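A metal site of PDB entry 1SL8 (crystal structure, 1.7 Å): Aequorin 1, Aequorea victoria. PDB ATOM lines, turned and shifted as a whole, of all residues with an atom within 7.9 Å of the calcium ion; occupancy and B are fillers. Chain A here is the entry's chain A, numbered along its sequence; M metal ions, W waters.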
ATOM      1  N   PHE A 115      -9.483 -20.117  20.610  1.00  0.00           N
ATOM      2  CA  PHE A 115     -10.199 -21.275  21.135  1.00  0.00           C
ATOM      3  C   PHE A 115     -10.812 -22.089  19.990  1.00  0.00           C
ATOM      4  O   PHE A 115     -10.691 -23.306  19.963  1.00  0.00           O
ATOM      5  CB  PHE A 115     -11.349 -20.828  22.032  1.00  0.00           C
ATOM      6  CG  PHE A 115     -11.982 -21.944  22.849  1.00  0.00           C
ATOM      7  CD1 PHE A 115     -11.566 -22.225  24.157  1.00  0.00           C
ATOM      8  CD2 PHE A 115     -13.033 -22.707  22.347  1.00  0.00           C
ATOM      9  CE1 PHE A 115     -12.176 -23.217  24.966  1.00  0.00           C
ATOM     10  CE2 PHE A 115     -13.622 -23.705  23.107  1.00  0.00           C
ATOM     11  CZ  PHE A 115     -13.213 -23.980  24.429  1.00  0.00           C
ATOM     12  N   ILE A 118      -8.079 -24.172  18.416  1.00  0.00           N
ATOM     13  CA  ILE A 118      -7.552 -25.339  19.126  1.00  0.00           C
ATOM     14  C   ILE A 118      -8.621 -26.409  19.403  1.00  0.00           C
ATOM     15  O   ILE A 118      -8.328 -27.571  19.642  1.00  0.00           O
ATOM     16  CB  ILE A 118      -6.803 -24.914  20.392  1.00  0.00           C
ATOM     17  CG1 ILE A 118      -7.637 -24.026  21.264  1.00  0.00           C
ATOM     18  CG2 ILE A 118      -5.595 -24.101  19.989  1.00  0.00           C
ATOM     19  CD1 ILE A 118      -6.865 -23.628  22.600  1.00  0.00           C
ATOM     20  N   ASP A 119      -9.876 -26.004  19.424  1.00  0.00           N
ATOM     21  CA  ASP A 119     -10.966 -26.942  19.532  1.00  0.00           C
ATOM     22  C   ASP A 119     -11.184 -27.670  18.197  1.00  0.00           C
ATOM     23  O   ASP A 119     -12.202 -27.466  17.486  1.00  0.00           O
ATOM     24  CB  ASP A 119     -12.225 -26.204  19.988  1.00  0.00           C
ATOM     25  CG  ASP A 119     -13.404 -27.136  20.189  1.00  0.00           C
ATOM     26  OD1 ASP A 119     -13.214 -28.357  20.454  1.00  0.00           O
ATOM     27  OD2 ASP A 119     -14.549 -26.650  20.109  1.00  0.00           O
ATOM     28  N   LYS A 120     -10.269 -28.578  17.903  1.00  0.00           N
ATOM     29  CA  LYS A 120     -10.351 -29.344  16.667  1.00  0.00           C
ATOM     30  C   LYS A 120     -11.668 -30.132  16.498  1.00  0.00           C
ATOM     31  O   LYS A 120     -12.188 -30.142  15.397  1.00  0.00           O
ATOM     32  CB  LYS A 120      -9.142 -30.262  16.519  1.00  0.00           C
ATOM     33  CG  LYS A 120      -7.949 -29.544  15.972  1.00  0.00           C
ATOM     34  CD  LYS A 120      -8.014 -29.358  14.430  1.00  0.00           C
ATOM     35  CE  LYS A 120      -6.663 -29.755  13.795  1.00  0.00           C
ATOM     36  NZ  LYS A 120      -6.493 -29.526  12.309  1.00  0.00           N
ATOM     37  N   ASP A 121     -12.213 -30.752  17.545  1.00  0.00           N
ATOM     38  CA  ASP A 121     -13.444 -31.578  17.370  1.00  0.00           C
ATOM     39  C   ASP A 121     -14.736 -30.749  17.491  1.00  0.00           C
ATOM     40  O   ASP A 121     -15.852 -31.314  17.535  1.00  0.00           O
ATOM     41  CB  ASP A 121     -13.484 -32.891  18.203  1.00  0.00           C
ATOM     42  CG  ASP A 121     -13.639 -32.679  19.726  1.00  0.00           C
ATOM     43  OD1 ASP A 121     -13.838 -31.539  20.180  1.00  0.00           O
ATOM     44  OD2 ASP A 121     -13.600 -33.627  20.554  1.00  0.00           O
ATOM     45  N   GLN A 122     -14.580 -29.421  17.523  1.00  0.00           N
ATOM     46  CA  GLN A 122     -15.725 -28.502  17.591  1.00  0.00           C
ATOM     47  C   GLN A 122     -16.818 -28.845  18.601  1.00  0.00           C
ATOM     48  O   GLN A 122     -17.990 -28.542  18.342  1.00  0.00           O
ATOM     49  CB  GLN A 122     -16.312 -28.183  16.195  1.00  0.00           C
ATOM     50  CG  GLN A 122     -15.292 -27.693  15.156  1.00  0.00           C
ATOM     51  CD  GLN A 122     -15.015 -26.179  15.218  1.00  0.00           C
ATOM     52  OE1 GLN A 122     -13.893 -25.716  15.554  1.00  0.00           O
ATOM     53  NE2 GLN A 122     -16.038 -25.400  14.918  1.00  0.00           N
ATOM     54  N   ASN A 123     -16.459 -29.461  19.727  1.00  0.00           N
ATOM     55  CA  ASN A 123     -17.400 -29.748  20.830  1.00  0.00           C
ATOM     56  C   ASN A 123     -17.504 -28.632  21.892  1.00  0.00           C
ATOM     57  O   ASN A 123     -18.185 -28.811  22.911  1.00  0.00           O
ATOM     58  CB  ASN A 123     -17.069 -31.090  21.506  1.00  0.00           C
ATOM     59  CG  ASN A 123     -15.968 -30.968  22.572  1.00  0.00           C
ATOM     60  OD1 ASN A 123     -15.048 -30.188  22.420  1.00  0.00           O
ATOM     61  ND2 ASN A 123     -16.104 -31.683  23.684  1.00  0.00           N
ATOM     62  N   GLY A 124     -16.751 -27.535  21.663  1.00  0.00           N
ATOM     63  CA  GLY A 124     -16.745 -26.366  22.533  1.00  0.00           C
ATOM     64  C   GLY A 124     -15.959 -26.533  23.832  1.00  0.00           C
ATOM     65  O   GLY A 124     -16.242 -25.866  24.807  1.00  0.00           O
ATOM     66  N   ALA A 125     -15.013 -27.471  23.852  1.00  0.00           N
ATOM     67  CA  ALA A 125     -14.205 -27.713  25.063  1.00  0.00           C
ATOM     68  C   ALA A 125     -12.862 -28.262  24.599  1.00  0.00           C
ATOM     69  O   ALA A 125     -12.766 -28.876  23.530  1.00  0.00           O
ATOM     70  CB  ALA A 125     -14.866 -28.672  25.944  1.00  0.00           C
ATOM     71  N   ILE A 126     -11.820 -28.010  25.385  1.00  0.00           N
ATOM     72  CA  ILE A 126     -10.481 -28.456  24.950  1.00  0.00           C
ATOM     73  C   ILE A 126     -10.138 -29.722  25.665  1.00  0.00           C
ATOM     74  O   ILE A 126     -10.012 -29.731  26.894  1.00  0.00           O
ATOM     75  CB  ILE A 126      -9.418 -27.334  25.281  1.00  0.00           C
ATOM     76  CG1 ILE A 126      -9.886 -25.948  24.730  1.00  0.00           C
ATOM     77  CG2 ILE A 126      -8.005 -27.773  24.782  1.00  0.00           C
ATOM     78  CD1 ILE A 126     -10.222 -25.791  23.239  1.00  0.00           C
ATOM     79  N   SER A 127      -9.960 -30.827  24.913  1.00  0.00           N
ATOM     80  CA  SER A 127      -9.502 -32.043  25.524  1.00  0.00           C
ATOM     81  C   SER A 127      -7.989 -31.946  25.856  1.00  0.00           C
ATOM     82  O   SER A 127      -7.290 -31.074  25.317  1.00  0.00           O
ATOM     83  CB  SER A 127      -9.660 -33.206  24.526  1.00  0.00           C
ATOM     84  OG  SER A 127      -8.795 -32.981  23.408  1.00  0.00           O
ATOM     85  N   LEU A 128      -7.514 -32.908  26.591  1.00  0.00           N
ATOM     86  CA  LEU A 128      -6.065 -33.049  26.811  1.00  0.00           C
ATOM     87  C   LEU A 128      -5.262 -33.115  25.523  1.00  0.00           C
ATOM     88  O   LEU A 128      -4.221 -32.460  25.385  1.00  0.00           O
ATOM     89  CB  LEU A 128      -5.767 -34.260  27.674  1.00  0.00           C
ATOM     90  CG  LEU A 128      -4.310 -34.550  28.017  1.00  0.00           C
ATOM     91  CD1 LEU A 128      -3.670 -33.338  28.805  1.00  0.00           C
ATOM     92  CD2 LEU A 128      -4.268 -35.822  28.857  1.00  0.00           C
ATOM     93  N   GLU A 130      -6.048 -31.923  22.658  1.00  0.00           N
ATOM     94  CA  GLU A 130      -6.128 -30.621  22.006  1.00  0.00           C
ATOM     95  C   GLU A 130      -5.151 -29.632  22.677  1.00  0.00           C
ATOM     96  O   GLU A 130      -4.535 -28.782  22.013  1.00  0.00           O
ATOM     97  CB  GLU A 130      -7.558 -30.093  22.036  1.00  0.00           C
ATOM     98  CG  GLU A 130      -8.419 -30.838  20.980  1.00  0.00           C
ATOM     99  CD  GLU A 130      -9.907 -30.550  21.107  1.00  0.00           C
ATOM    100  OE1 GLU A 130     -10.343 -30.016  22.178  1.00  0.00           O
ATOM    101  OE2 GLU A 130     -10.658 -30.855  20.124  1.00  0.00           O
ATOM    102  N   GLN A 161     -12.113 -31.482  30.626  1.00  0.00           N
ATOM    103  CA  GLN A 161     -11.903 -30.630  29.469  1.00  0.00           C
ATOM    104  C   GLN A 161     -11.953 -29.166  29.825  1.00  0.00           C
ATOM    105  O   GLN A 161     -12.508 -28.768  30.859  1.00  0.00           O
ATOM    106  CB  GLN A 161     -12.979 -30.844  28.406  1.00  0.00           C
ATOM    107  CG  GLN A 161     -12.947 -32.227  27.809  1.00  0.00           C
ATOM    108  CD  GLN A 161     -13.842 -32.255  26.537  1.00  0.00           C
ATOM    109  OE1 GLN A 161     -13.431 -31.889  25.442  1.00  0.00           O
ATOM    110  NE2 GLN A 161     -15.109 -32.632  26.739  1.00  0.00           N
ATOM    111  N   LEU A 162     -11.333 -28.365  28.940  1.00  0.00           N
ATOM    112  CA  LEU A 162     -11.210 -26.941  29.283  1.00  0.00           C
ATOM    113  C   LEU A 162     -12.230 -26.123  28.545  1.00  0.00           C
ATOM    114  O   LEU A 162     -12.273 -26.116  27.288  1.00  0.00           O
ATOM    115  CB  LEU A 162      -9.784 -26.361  29.067  1.00  0.00           C
ATOM    116  CG  LEU A 162      -8.663 -27.302  29.496  1.00  0.00           C
ATOM    117  CD1 LEU A 162      -7.268 -26.636  29.010  1.00  0.00           C
ATOM    118  CD2 LEU A 162      -8.622 -27.533  30.957  1.00  0.00           C
HETATM  119 CA    CA M   1     -12.700 -30.197  21.618  1.00  0.00          CA
HETATM  120  O   HOH W   1     -12.547 -32.242  23.217  1.00  0.00           O
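The side-chain amide oxygen (OE1) of Gln 122 lies close to the backbone carbonyl oxygen (O) of Asp 119. The side-chain carboxylate of Asp 119 sits at hydrogen-bond distance from the backbone NH of Gly 124 (2.8 Å). The side-chain carboxylate of Glu 130 sits close to the backbone NH of Lys 120, 3.2 Å away. The backbone NH (N) of Glu 130 is in hydrogen-bond range of the side-chain hydroxyl (OG) of Ser 127 (3.0 Å). The side-chain amide nitrogen (ND2) of Asn 123 is in hydrogen-bond range of the side-chain amide oxygen (OE1) of Gln 161, 3.2 Å away.
Of the 15 residues printed, 5 come within 4 Å of the calcium ion. The nearest printed residue that does not touch the calcium ion is Gln 161 (4.2 Å).
The calcium ion is bound by OD1 of Asp 119 (2.2 Å), OD1 of Asp 121 (2.3 Å), O of Ala 125 (2.3 Å), OE1 of Glu 130 (2.4 Å), OD1 of Asn 123 (2.5 Å), water W1 (2.6 Å) and OE2 of Glu 130 (2.6 Å). The calcium ion has seven donor atoms within binding distance.
Water W1 lies within hydrogen-bond range of OE1 of Gln 161 (2.4 Å), OD2 of Asp 121 (3.2 Å) and N of Ser 127 (3.4 Å).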
